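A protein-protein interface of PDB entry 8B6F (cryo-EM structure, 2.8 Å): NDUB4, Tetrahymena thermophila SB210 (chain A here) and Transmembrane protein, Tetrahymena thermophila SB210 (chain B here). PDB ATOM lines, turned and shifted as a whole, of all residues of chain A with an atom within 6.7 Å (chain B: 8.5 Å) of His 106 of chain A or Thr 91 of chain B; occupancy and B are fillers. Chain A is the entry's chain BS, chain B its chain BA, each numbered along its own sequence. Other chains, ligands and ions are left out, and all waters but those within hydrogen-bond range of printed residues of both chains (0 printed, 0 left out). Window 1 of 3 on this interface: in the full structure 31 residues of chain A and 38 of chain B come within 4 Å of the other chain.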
ATOM      1  N   ILE A 101      -7.030   6.226  20.431  1.00  0.00           N
ATOM      2  CA  ILE A 101      -5.665   5.809  20.740  1.00  0.00           C
ATOM      3  C   ILE A 101      -5.658   4.396  21.311  1.00  0.00           C
ATOM      4  O   ILE A 101      -4.807   3.573  20.958  1.00  0.00           O
ATOM      5  CB  ILE A 101      -5.005   6.817  21.700  1.00  0.00           C
ATOM      6  CG1 ILE A 101      -4.760   8.146  20.980  1.00  0.00           C
ATOM      7  CG2 ILE A 101      -3.695   6.264  22.253  1.00  0.00           C
ATOM      8  CD1 ILE A 101      -4.315   9.273  21.891  1.00  0.00           C
ATOM      9  N   LEU A 102      -6.602   4.094  22.204  1.00  0.00           N
ATOM     10  CA  LEU A 102      -6.660   2.758  22.787  1.00  0.00           C
ATOM     11  C   LEU A 102      -6.976   1.707  21.731  1.00  0.00           C
ATOM     12  O   LEU A 102      -6.393   0.617  21.736  1.00  0.00           O
ATOM     13  CB  LEU A 102      -7.697   2.715  23.909  1.00  0.00           C
ATOM     14  CG  LEU A 102      -7.369   3.509  25.177  1.00  0.00           C
ATOM     15  CD1 LEU A 102      -8.523   3.429  26.160  1.00  0.00           C
ATOM     16  CD2 LEU A 102      -6.085   3.018  25.827  1.00  0.00           C
ATOM     17  N   HIS A 103      -7.897   2.014  20.817  1.00  0.00           N
ATOM     18  CA  HIS A 103      -8.212   1.072  19.748  1.00  0.00           C
ATOM     19  C   HIS A 103      -6.987   0.814  18.881  1.00  0.00           C
ATOM     20  O   HIS A 103      -6.681  -0.335  18.542  1.00  0.00           O
ATOM     21  CB  HIS A 103      -9.371   1.607  18.908  1.00  0.00           C
ATOM     22  CG  HIS A 103      -9.806   0.678  17.819  1.00  0.00           C
ATOM     23  ND1 HIS A 103     -10.387  -0.547  18.072  1.00  0.00           N
ATOM     24  CD2 HIS A 103      -9.750   0.796  16.471  1.00  0.00           C
ATOM     25  CE1 HIS A 103     -10.668  -1.142  16.927  1.00  0.00           C
ATOM     26  NE2 HIS A 103     -10.291  -0.351  15.941  1.00  0.00           N
ATOM     27  N   ARG A 104      -6.274   1.877  18.510  1.00  0.00           N
ATOM     28  CA  ARG A 104      -5.057   1.715  17.724  1.00  0.00           C
ATOM     29  C   ARG A 104      -4.027   0.888  18.483  1.00  0.00           C
ATOM     30  O   ARG A 104      -3.359   0.026  17.901  1.00  0.00           O
ATOM     31  CB  ARG A 104      -4.486   3.084  17.354  1.00  0.00           C
ATOM     32  CG  ARG A 104      -3.269   3.020  16.443  1.00  0.00           C
ATOM     33  CD  ARG A 104      -2.730   4.408  16.140  1.00  0.00           C
ATOM     34  NE  ARG A 104      -2.265   5.089  17.341  1.00  0.00           N
ATOM     35  CZ  ARG A 104      -1.721   6.297  17.355  1.00  0.00           C
ATOM     36  NH1 ARG A 104      -1.555   6.994  16.243  1.00  0.00           N
ATOM     37  NH2 ARG A 104      -1.332   6.821  18.514  1.00  0.00           N
ATOM     38  N   GLU A 105      -3.890   1.135  19.786  1.00  0.00           N
ATOM     39  CA  GLU A 105      -2.934   0.380  20.589  1.00  0.00           C
ATOM     40  C   GLU A 105      -3.296  -1.098  20.639  1.00  0.00           C
ATOM     41  O   GLU A 105      -2.413  -1.961  20.587  1.00  0.00           O
ATOM     42  CB  GLU A 105      -2.865   0.964  22.001  1.00  0.00           C
ATOM     43  CG  GLU A 105      -2.129   0.090  23.010  1.00  0.00           C
ATOM     44  CD  GLU A 105      -0.750  -0.326  22.534  1.00  0.00           C
ATOM     45  OE1 GLU A 105      -0.180   0.374  21.671  1.00  0.00           O
ATOM     46  OE2 GLU A 105      -0.237  -1.354  23.021  1.00  0.00           O
ATOM     47  N   HIS A 106      -4.587  -1.414  20.743  1.00  0.00           N
ATOM     48  CA  HIS A 106      -4.997  -2.813  20.788  1.00  0.00           C
ATOM     49  C   HIS A 106      -4.674  -3.520  19.478  1.00  0.00           C
ATOM     50  O   HIS A 106      -4.149  -4.640  19.479  1.00  0.00           O
ATOM     51  CB  HIS A 106      -6.489  -2.909  21.100  1.00  0.00           C
ATOM     52  CG  HIS A 106      -6.858  -2.359  22.442  1.00  0.00           C
ATOM     53  ND1 HIS A 106      -8.165  -2.238  22.864  1.00  0.00           N
ATOM     54  CD2 HIS A 106      -6.092  -1.900  23.460  1.00  0.00           C
ATOM     55  CE1 HIS A 106      -8.187  -1.726  24.081  1.00  0.00           C
ATOM     56  NE2 HIS A 106      -6.942  -1.513  24.467  1.00  0.00           N
ATOM     57  N   ASN A 107      -4.981  -2.885  18.344  1.00  0.00           N
ATOM     58  CA  ASN A 107      -4.657  -3.495  17.059  1.00  0.00           C
ATOM     59  C   ASN A 107      -3.153  -3.671  16.908  1.00  0.00           C
ATOM     60  O   ASN A 107      -2.680  -4.718  16.454  1.00  0.00           O
ATOM     61  CB  ASN A 107      -5.215  -2.648  15.919  1.00  0.00           C
ATOM     62  CG  ASN A 107      -6.718  -2.498  15.990  1.00  0.00           C
ATOM     63  OD1 ASN A 107      -7.323  -2.696  17.043  1.00  0.00           O
ATOM     64  ND2 ASN A 107      -7.332  -2.148  14.867  1.00  0.00           N
ATOM     65  N   GLU A 108      -2.383  -2.648  17.284  1.00  0.00           N
ATOM     66  CA  GLU A 108      -0.931  -2.743  17.206  1.00  0.00           C
ATOM     67  C   GLU A 108      -0.406  -3.843  18.118  1.00  0.00           C
ATOM     68  O   GLU A 108       0.551  -4.544  17.771  1.00  0.00           O
ATOM     69  CB  GLU A 108      -0.298  -1.400  17.568  1.00  0.00           C
ATOM     70  CG  GLU A 108      -0.561  -0.301  16.549  1.00  0.00           C
ATOM     71  CD  GLU A 108      -0.079   1.058  17.020  1.00  0.00           C
ATOM     72  OE1 GLU A 108       0.353   1.166  18.186  1.00  0.00           O
ATOM     73  OE2 GLU A 108      -0.129   2.019  16.223  1.00  0.00           O
ATOM     74  N   HIS A 109      -1.026  -4.014  19.287  1.00  0.00           N
ATOM     75  CA  HIS A 109      -0.602  -5.066  20.203  1.00  0.00           C
ATOM     76  C   HIS A 109      -0.844  -6.448  19.612  1.00  0.00           C
ATOM     77  O   HIS A 109       0.012  -7.333  19.723  1.00  0.00           O
ATOM     78  CB  HIS A 109      -1.330  -4.922  21.540  1.00  0.00           C
ATOM     79  CG  HIS A 109      -1.036  -6.024  22.509  1.00  0.00           C
ATOM     80  ND1 HIS A 109       0.245  -6.335  22.915  1.00  0.00           N
ATOM     81  CD2 HIS A 109      -1.854  -6.890  23.152  1.00  0.00           C
ATOM     82  CE1 HIS A 109       0.201  -7.344  23.767  1.00  0.00           C
ATOM     83  NE2 HIS A 109      -1.061  -7.699  23.928  1.00  0.00           N
ATOM     84  N   LYS A 110      -1.998  -6.657  18.978  1.00  0.00           N
ATOM     85  CA  LYS A 110      -2.252  -7.942  18.335  1.00  0.00           C
ATOM     86  C   LYS A 110      -1.217  -8.215  17.254  1.00  0.00           C
ATOM     87  O   LYS A 110      -0.659  -9.314  17.176  1.00  0.00           O
ATOM     88  CB  LYS A 110      -3.663  -7.964  17.752  1.00  0.00           C
ATOM     89  CG  LYS A 110      -4.758  -7.990  18.806  1.00  0.00           C
ATOM     90  CD  LYS A 110      -6.149  -7.941  18.187  1.00  0.00           C
ATOM     91  CE  LYS A 110      -6.405  -9.119  17.261  1.00  0.00           C
ATOM     92  NZ  LYS A 110      -6.115 -10.429  17.905  1.00  0.00           N
ATOM     93  N   LEU A 111      -0.949  -7.224  16.402  1.00  0.00           N
ATOM     94  CA  LEU A 111       0.044  -7.416  15.353  1.00  0.00           C
ATOM     95  C   LEU A 111       1.424  -7.663  15.946  1.00  0.00           C
ATOM     96  O   LEU A 111       2.182  -8.503  15.449  1.00  0.00           O
ATOM     97  CB  LEU A 111       0.080  -6.217  14.409  1.00  0.00           C
ATOM     98  CG  LEU A 111       1.161  -6.402  13.343  1.00  0.00           C
ATOM     99  CD1 LEU A 111       0.626  -6.161  11.965  1.00  0.00           C
ATOM    100  CD2 LEU A 111       2.326  -5.461  13.620  1.00  0.00           C
ATOM    101  N   ILE B  26      -0.777  -4.677   9.500  1.00  0.00           N
ATOM    102  CA  ILE B  26      -2.097  -5.168   9.893  1.00  0.00           C
ATOM    103  C   ILE B  26      -2.932  -5.464   8.655  1.00  0.00           C
ATOM    104  O   ILE B  26      -3.544  -6.533   8.536  1.00  0.00           O
ATOM    105  CB  ILE B  26      -2.806  -4.153  10.811  1.00  0.00           C
ATOM    106  CG1 ILE B  26      -2.125  -4.082  12.179  1.00  0.00           C
ATOM    107  CG2 ILE B  26      -4.282  -4.516  10.986  1.00  0.00           C
ATOM    108  CD1 ILE B  26      -2.585  -2.935  13.047  1.00  0.00           C
ATOM    109  N   TYR B  33      -4.053 -13.911  11.635  1.00  0.00           N
ATOM    110  CA  TYR B  33      -4.238 -13.875  13.080  1.00  0.00           C
ATOM    111  C   TYR B  33      -5.579 -13.293  13.503  1.00  0.00           C
ATOM    112  O   TYR B  33      -5.832 -13.185  14.707  1.00  0.00           O
ATOM    113  CB  TYR B  33      -3.110 -13.072  13.734  1.00  0.00           C
ATOM    114  CG  TYR B  33      -3.215 -11.576  13.538  1.00  0.00           C
ATOM    115  CD1 TYR B  33      -2.648 -10.960  12.432  1.00  0.00           C
ATOM    116  CD2 TYR B  33      -3.872 -10.780  14.465  1.00  0.00           C
ATOM    117  CE1 TYR B  33      -2.738  -9.593  12.251  1.00  0.00           C
ATOM    118  CE2 TYR B  33      -3.968  -9.414  14.295  1.00  0.00           C
ATOM    119  CZ  TYR B  33      -3.399  -8.826  13.187  1.00  0.00           C
ATOM    120  OH  TYR B  33      -3.493  -7.466  13.016  1.00  0.00           O
ATOM    121  N   HIS B  56      -9.311   1.646  11.382  1.00  0.00           N
ATOM    122  CA  HIS B  56      -8.047   1.652  12.118  1.00  0.00           C
ATOM    123  C   HIS B  56      -7.265   2.898  11.723  1.00  0.00           C
ATOM    124  O   HIS B  56      -6.437   2.884  10.811  1.00  0.00           O
ATOM    125  CB  HIS B  56      -7.256   0.382  11.832  1.00  0.00           C
ATOM    126  CG  HIS B  56      -5.877   0.386  12.414  1.00  0.00           C
ATOM    127  ND1 HIS B  56      -5.641   0.484  13.769  1.00  0.00           N
ATOM    128  CD2 HIS B  56      -4.661   0.301  11.826  1.00  0.00           C
ATOM    129  CE1 HIS B  56      -4.339   0.463  13.988  1.00  0.00           C
ATOM    130  NE2 HIS B  56      -3.721   0.352  12.827  1.00  0.00           N
ATOM    131  N   PHE B  84      -8.747   6.619  34.791  1.00  0.00           N
ATOM    132  CA  PHE B  84      -8.578   6.460  33.352  1.00  0.00           C
ATOM    133  C   PHE B  84      -7.102   6.448  32.977  1.00  0.00           C
ATOM    134  O   PHE B  84      -6.680   5.684  32.101  1.00  0.00           O
ATOM    135  CB  PHE B  84      -9.309   7.573  32.605  1.00  0.00           C
ATOM    136  CG  PHE B  84      -9.357   7.366  31.123  1.00  0.00           C
ATOM    137  CD1 PHE B  84      -8.321   7.801  30.315  1.00  0.00           C
ATOM    138  CD2 PHE B  84     -10.434   6.722  30.540  1.00  0.00           C
ATOM    139  CE1 PHE B  84      -8.363   7.605  28.948  1.00  0.00           C
ATOM    140  CE2 PHE B  84     -10.484   6.523  29.175  1.00  0.00           C
ATOM    141  CZ  PHE B  84      -9.448   6.965  28.378  1.00  0.00           C
ATOM    142  N   ALA B  85      -6.298   7.293  33.628  1.00  0.00           N
ATOM    143  CA  ALA B  85      -4.865   7.307  33.354  1.00  0.00           C
ATOM    144  C   ALA B  85      -4.222   5.981  33.724  1.00  0.00           C
ATOM    145  O   ALA B  85      -3.376   5.464  32.987  1.00  0.00           O
ATOM    146  CB  ALA B  85      -4.194   8.442  34.123  1.00  0.00           C
ATOM    147  N   LEU B  86      -4.618   5.406  34.860  1.00  0.00           N
ATOM    148  CA  LEU B  86      -4.099   4.097  35.237  1.00  0.00           C
ATOM    149  C   LEU B  86      -4.483   3.045  34.206  1.00  0.00           C
ATOM    150  O   LEU B  86      -3.668   2.186  33.853  1.00  0.00           O
ATOM    151  CB  LEU B  86      -4.617   3.712  36.622  1.00  0.00           C
ATOM    152  CG  LEU B  86      -4.164   4.602  37.784  1.00  0.00           C
ATOM    153  CD1 LEU B  86      -4.947   4.257  39.037  1.00  0.00           C
ATOM    154  CD2 LEU B  86      -2.670   4.470  38.036  1.00  0.00           C
ATOM    155  N   LYS B  87      -5.722   3.094  33.711  1.00  0.00           N
ATOM    156  CA  LYS B  87      -6.135   2.163  32.666  1.00  0.00           C
ATOM    157  C   LYS B  87      -5.279   2.333  31.419  1.00  0.00           C
ATOM    158  O   LYS B  87      -4.860   1.346  30.803  1.00  0.00           O
ATOM    159  CB  LYS B  87      -7.612   2.368  32.331  1.00  0.00           C
ATOM    160  CG  LYS B  87      -8.082   1.587  31.111  1.00  0.00           C
ATOM    161  CD  LYS B  87      -9.555   1.822  30.834  1.00  0.00           C
ATOM    162  CE  LYS B  87      -9.979   1.147  29.540  1.00  0.00           C
ATOM    163  NZ  LYS B  87     -11.419   1.378  29.237  1.00  0.00           N
ATOM    164  N   LYS B  88      -5.017   3.580  31.025  1.00  0.00           N
ATOM    165  CA  LYS B  88      -4.198   3.831  29.845  1.00  0.00           C
ATOM    166  C   LYS B  88      -2.780   3.309  30.043  1.00  0.00           C
ATOM    167  O   LYS B  88      -2.201   2.700  29.136  1.00  0.00           O
ATOM    168  CB  LYS B  88      -4.189   5.326  29.529  1.00  0.00           C
ATOM    169  CG  LYS B  88      -3.501   5.688  28.222  1.00  0.00           C
ATOM    170  CD  LYS B  88      -3.539   7.191  27.994  1.00  0.00           C
ATOM    171  CE  LYS B  88      -2.810   7.582  26.718  1.00  0.00           C
ATOM    172  NZ  LYS B  88      -2.831   9.054  26.504  1.00  0.00           N
ATOM    173  N   ILE B  89      -2.206   3.534  31.227  1.00  0.00           N
ATOM    174  CA  ILE B  89      -0.866   3.029  31.515  1.00  0.00           C
ATOM    175  C   ILE B  89      -0.846   1.512  31.422  1.00  0.00           C
ATOM    176  O   ILE B  89       0.063   0.920  30.830  1.00  0.00           O
ATOM    177  CB  ILE B  89      -0.405   3.500  32.906  1.00  0.00           C
ATOM    178  CG1 ILE B  89      -0.326   5.021  32.977  1.00  0.00           C
ATOM    179  CG2 ILE B  89       0.962   2.913  33.242  1.00  0.00           C
ATOM    180  CD1 ILE B  89      -0.343   5.550  34.391  1.00  0.00           C
ATOM    181  N   LYS B  90      -1.852   0.858  32.001  1.00  0.00           N
ATOM    182  CA  LYS B  90      -1.925  -0.596  31.928  1.00  0.00           C
ATOM    183  C   LYS B  90      -2.024  -1.072  30.487  1.00  0.00           C
ATOM    184  O   LYS B  90      -1.371  -2.046  30.100  1.00  0.00           O
ATOM    185  CB  LYS B  90      -3.122  -1.097  32.732  1.00  0.00           C
ATOM    186  CG  LYS B  90      -3.354  -2.583  32.598  1.00  0.00           C
ATOM    187  CD  LYS B  90      -4.469  -3.038  33.497  1.00  0.00           C
ATOM    188  CE  LYS B  90      -4.656  -4.528  33.379  1.00  0.00           C
ATOM    189  NZ  LYS B  90      -5.678  -5.008  34.325  1.00  0.00           N
ATOM    190  N   THR B  91      -2.840  -0.400  29.676  1.00  0.00           N
ATOM    191  CA  THR B  91      -2.995  -0.810  28.286  1.00  0.00           C
ATOM    192  C   THR B  91      -1.682  -0.692  27.524  1.00  0.00           C
ATOM    193  O   THR B  91      -1.348  -1.564  26.714  1.00  0.00           O
ATOM    194  CB  THR B  91      -4.081   0.031  27.614  1.00  0.00           C
ATOM    195  OG1 THR B  91      -5.342  -0.208  28.252  1.00  0.00           O
ATOM    196  CG2 THR B  91      -4.199  -0.310  26.134  1.00  0.00           C
ATOM    197  N   PHE B  92      -0.921   0.377  27.765  1.00  0.00           N
ATOM    198  CA  PHE B  92       0.274   0.620  26.964  1.00  0.00           C
ATOM    199  C   PHE B  92       1.459  -0.217  27.436  1.00  0.00           C
ATOM    200  O   PHE B  92       2.168  -0.809  26.616  1.00  0.00           O
ATOM    201  CB  PHE B  92       0.610   2.109  26.977  1.00  0.00           C
ATOM    202  CG  PHE B  92      -0.117   2.891  25.922  1.00  0.00           C
ATOM    203  CD1 PHE B  92       0.397   2.990  24.640  1.00  0.00           C
ATOM    204  CD2 PHE B  92      -1.325   3.505  26.204  1.00  0.00           C
ATOM    205  CE1 PHE B  92      -0.272   3.701  23.665  1.00  0.00           C
ATOM    206  CE2 PHE B  92      -1.999   4.217  25.234  1.00  0.00           C
ATOM    207  CZ  PHE B  92      -1.472   4.314  23.962  1.00  0.00           C
ATOM    208  N   ASN B  93       1.701  -0.275  28.745  1.00  0.00           N
ATOM    209  CA  ASN B  93       2.748  -1.129  29.295  1.00  0.00           C
ATOM    210  C   ASN B  93       2.143  -2.035  30.356  1.00  0.00           C
ATOM    211  O   ASN B  93       1.506  -1.556  31.299  1.00  0.00           O
ATOM    212  CB  ASN B  93       3.906  -0.312  29.886  1.00  0.00           C
ATOM    213  CG  ASN B  93       3.438   0.837  30.746  1.00  0.00           C
ATOM    214  OD1 ASN B  93       2.476   1.524  30.418  1.00  0.00           O
ATOM    215  ND2 ASN B  93       4.132   1.060  31.855  1.00  0.00           N
ATOM    216  N   HIS B  94       2.351  -3.341  30.198  1.00  0.00           N
ATOM    217  CA  HIS B  94       1.718  -4.342  31.044  1.00  0.00           C
ATOM    218  C   HIS B  94       2.516  -4.671  32.298  1.00  0.00           C
ATOM    219  O   HIS B  94       2.005  -5.386  33.166  1.00  0.00           O
ATOM    220  CB  HIS B  94       1.486  -5.629  30.245  1.00  0.00           C
ATOM    221  CG  HIS B  94       0.711  -5.423  28.981  1.00  0.00           C
ATOM    222  ND1 HIS B  94       1.219  -4.736  27.900  1.00  0.00           N
ATOM    223  CD2 HIS B  94      -0.536  -5.810  28.627  1.00  0.00           C
ATOM    224  CE1 HIS B  94       0.318  -4.711  26.934  1.00  0.00           C
ATOM    225  NE2 HIS B  94      -0.756  -5.356  27.350  1.00  0.00           N
ATOM    226  N   ASP B  95       3.744  -4.176  32.418  1.00  0.00           N
ATOM    227  CA  ASP B  95       4.572  -4.441  33.587  1.00  0.00           C
ATOM    228  C   ASP B  95       4.436  -3.370  34.661  1.00  0.00           C
ATOM    229  O   ASP B  95       5.122  -3.450  35.685  1.00  0.00           O
ATOM    230  CB  ASP B  95       6.041  -4.562  33.171  1.00  0.00           C
ATOM    231  CG  ASP B  95       6.253  -5.591  32.076  1.00  0.00           C
ATOM    232  OD1 ASP B  95       5.254  -6.168  31.600  1.00  0.00           O
ATOM    233  OD2 ASP B  95       7.418  -5.824  31.691  1.00  0.00           O
ATOM    234  N   PHE B  96       3.572  -2.374  34.456  1.00  0.00           N
ATOM    235  CA  PHE B  96       3.462  -1.281  35.415  1.00  0.00           C
ATOM    236  C   PHE B  96       2.797  -1.735  36.709  1.00  0.00           C
ATOM    237  O   PHE B  96       3.251  -1.378  37.802  1.00  0.00           O
ATOM    238  CB  PHE B  96       2.681  -0.123  34.792  1.00  0.00           C
ATOM    239  CG  PHE B  96       2.762   1.156  35.575  1.00  0.00           C
ATOM    240  CD1 PHE B  96       1.904   1.392  36.636  1.00  0.00           C
ATOM    241  CD2 PHE B  96       3.691   2.126  35.241  1.00  0.00           C
ATOM    242  CE1 PHE B  96       1.976   2.569  37.354  1.00  0.00           C
ATOM    243  CE2 PHE B  96       3.767   3.305  35.954  1.00  0.00           C
ATOM    244  CZ  PHE B  96       2.909   3.527  37.012  1.00  0.00           C
ATOM    245  N   PHE B  97       1.727  -2.517  36.609  1.00  0.00           N
ATOM    246  CA  PHE B  97       0.902  -2.872  37.753  1.00  0.00           C
ATOM    247  C   PHE B  97       1.153  -4.314  38.176  1.00  0.00           C
ATOM    248  O   PHE B  97       1.545  -5.160  37.368  1.00  0.00           O
ATOM    249  CB  PHE B  97      -0.584  -2.684  37.433  1.00  0.00           C
ATOM    250  CG  PHE B  97      -0.959  -1.267  37.113  1.00  0.00           C
ATOM    251  CD1 PHE B  97      -1.285  -0.379  38.124  1.00  0.00           C
ATOM    252  CD2 PHE B  97      -0.984  -0.822  35.803  1.00  0.00           C
ATOM    253  CE1 PHE B  97      -1.630   0.925  37.835  1.00  0.00           C
ATOM    254  CE2 PHE B  97      -1.328   0.482  35.506  1.00  0.00           C
ATOM    255  CZ  PHE B  97      -1.653   1.358  36.523  1.00  0.00           C
ATOM    256  N   GLU B 102      -3.845  -5.217  38.546  1.00  0.00           N
ATOM    257  CA  GLU B 102      -4.358  -5.598  37.236  1.00  0.00           C
ATOM    258  C   GLU B 102      -5.756  -6.191  37.346  1.00  0.00           C
ATOM    259  O   GLU B 102      -6.631  -5.896  36.524  1.00  0.00           O
ATOM    260  CB  GLU B 102      -3.409  -6.585  36.555  1.00  0.00           C
ATOM    261  CG  GLU B 102      -2.144  -5.942  36.012  1.00  0.00           C
ATOM    262  CD  GLU B 102      -1.273  -6.925  35.253  1.00  0.00           C
ATOM    263  OE1 GLU B 102      -1.586  -8.133  35.266  1.00  0.00           O
ATOM    264  OE2 GLU B 102      -0.279  -6.487  34.637  1.00  0.00           O
ATOM    265  N   LEU B 105      -8.190  -3.379  37.847  1.00  0.00           N
ATOM    266  CA  LEU B 105      -8.442  -2.583  36.651  1.00  0.00           C
ATOM    267  C   LEU B 105      -9.244  -3.349  35.604  1.00  0.00           C
ATOM    268  O   LEU B 105     -10.006  -2.738  34.847  1.00  0.00           O
ATOM    269  CB  LEU B 105      -7.116  -2.104  36.061  1.00  0.00           C
ATOM    270  CG  LEU B 105      -6.332  -1.099  36.912  1.00  0.00           C
ATOM    271  CD1 LEU B 105      -4.965  -0.835  36.309  1.00  0.00           C
ATOM    272  CD2 LEU B 105      -7.098   0.204  37.073  1.00  0.00           C
ATOM    273  N   LEU B 202       5.138   6.562  27.690  1.00  0.00           N
ATOM    274  CA  LEU B 202       4.205   5.811  28.521  1.00  0.00           C
ATOM    275  C   LEU B 202       4.552   4.326  28.523  1.00  0.00           C
ATOM    276  O   LEU B 202       4.496   3.669  29.570  1.00  0.00           O
ATOM    277  CB  LEU B 202       2.779   6.033  28.018  1.00  0.00           C
ATOM    278  CG  LEU B 202       1.644   5.591  28.940  1.00  0.00           C
ATOM    279  CD1 LEU B 202       1.679   6.389  30.227  1.00  0.00           C
ATOM    280  CD2 LEU B 202       0.302   5.748  28.261  1.00  0.00           C
ATOM    281  N   ARG B 203       4.909   3.778  27.358  1.00  0.00           N
ATOM    282  CA  ARG B 203       5.303   2.373  27.287  1.00  0.00           C
ATOM    283  C   ARG B 203       6.537   2.101  28.136  1.00  0.00           C
ATOM    284  O   ARG B 203       6.599   1.093  28.850  1.00  0.00           O
ATOM    285  CB  ARG B 203       5.574   1.975  25.837  1.00  0.00           C
ATOM    286  CG  ARG B 203       4.349   1.949  24.944  1.00  0.00           C
ATOM    287  CD  ARG B 203       4.761   1.832  23.484  1.00  0.00           C
ATOM    288  NE  ARG B 203       3.612   1.767  22.588  1.00  0.00           N
ATOM    289  CZ  ARG B 203       3.009   0.646  22.217  1.00  0.00           C
ATOM    290  NH1 ARG B 203       3.406  -0.535  22.663  1.00  0.00           N
ATOM    291  NH2 ARG B 203       1.981   0.710  21.376  1.00  0.00           N
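O of His 103 of chain A lies close to OD1 of Asn 107 of chain A (2.9 Å).
NE of Arg 104 of chain A lies within salt-bridge range of OE2 of Glu 108 of chain A (3.9 Å).
The side-chain hydroxyl (OG1) of Thr 91 of chain B sits at hydrogen-bond distance from the backbone carbonyl oxygen (O) of Lys 87 of chain B, at 3.0 Å.
Phe 92 of chain B touches Ile 101 of chain A.
CD2 of Leu 102 of chain A touches CG2 of Thr 91 of chain B, 3.8 Å away.
CE1 of His 56 of chain B touches CG of Arg 104 of chain A, at 3.7 Å.
Thr 91 of chain B touches Glu 105 of chain A (CG2 to CG, 3.8 Å).
Phe 92 of chain B touches Glu 105 of chain A (CE1 to OE1, 3.9 Å).
Thr 91 of chain B touches His 106 of chain A (CG2 to NE2, 3.4 Å).
Ile 26 of chain B touches Asn 107 of chain A.
CB of Lys 110 of chain A touches CE2 of Tyr 33 of chain B (3.8 Å).
Leu 111 of chain A touches Ile 26 of chain B (CD1 to N, 3.2 Å).
The guanidinium group of Arg 203 of chain B is in salt-bridge range of the side-chain carboxylate of Glu 108 of chain A, 3.6 Å away.
The side-chain amide nitrogen of Asn 107 of chain A is in hydrogen-bond range of a ring nitrogen (ND1) of His 56 of chain B (3.3 Å).
NH2 of Arg 203 of chain B lies within salt-bridge range of OE2 of Glu 105 of chain A.
Of the 21 printed residues of chain B, 6 touch a printed residue of chain A.
Hydrophobic or aromatic side chains of chain B within 4 Å of the printed part of chain A: Ile 26, Tyr 33, His 56 and Phe 92.
Of the 11 printed residues of chain A, 9 touch a printed residue of chain B.
Printed residues of chain A that touch a printed residue of chain B: Ile 101, Leu 102, Arg 104, Glu 105, His 106, Asn 107, Glu 108, Lys 110 and Leu 111.
Hydrophobic or aromatic side chains of chain A within 4 Å of the printed part of chain B: Ile 101, Leu 102, His 106 and Leu 111.
Among the printed residues, 12 pairs touch across the chains.
Among the printed residues, Asp or Glu carboxylates within 4 Å of a Lys or Arg side-chain nitrogen of the other chain: Glu 105 of chain A with Arg 203 of chain B and Glu 108 of chain A with Arg 203 of chain B.
Printed residues of chain B within 4 Å of Arg 104 of chain A: His 56 (3.7 Å).
His 106 of chain A touches just one residue of chain B: Thr 91.
Printed residues of chain B within 4 Å of Asn 107 of chain A: Ile 26 (3.8 Å) and His 56 (3.3 Å).
Of the printed residues of chain B, Leu 111 of chain A touches Ile 26 (3.2 Å).
Thr 91 of chain B touches three residues of chain A.
The nearest printed residue of chain B that does not touch Leu 111 of chain A is Tyr 33 of chain B (4.03 Å).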
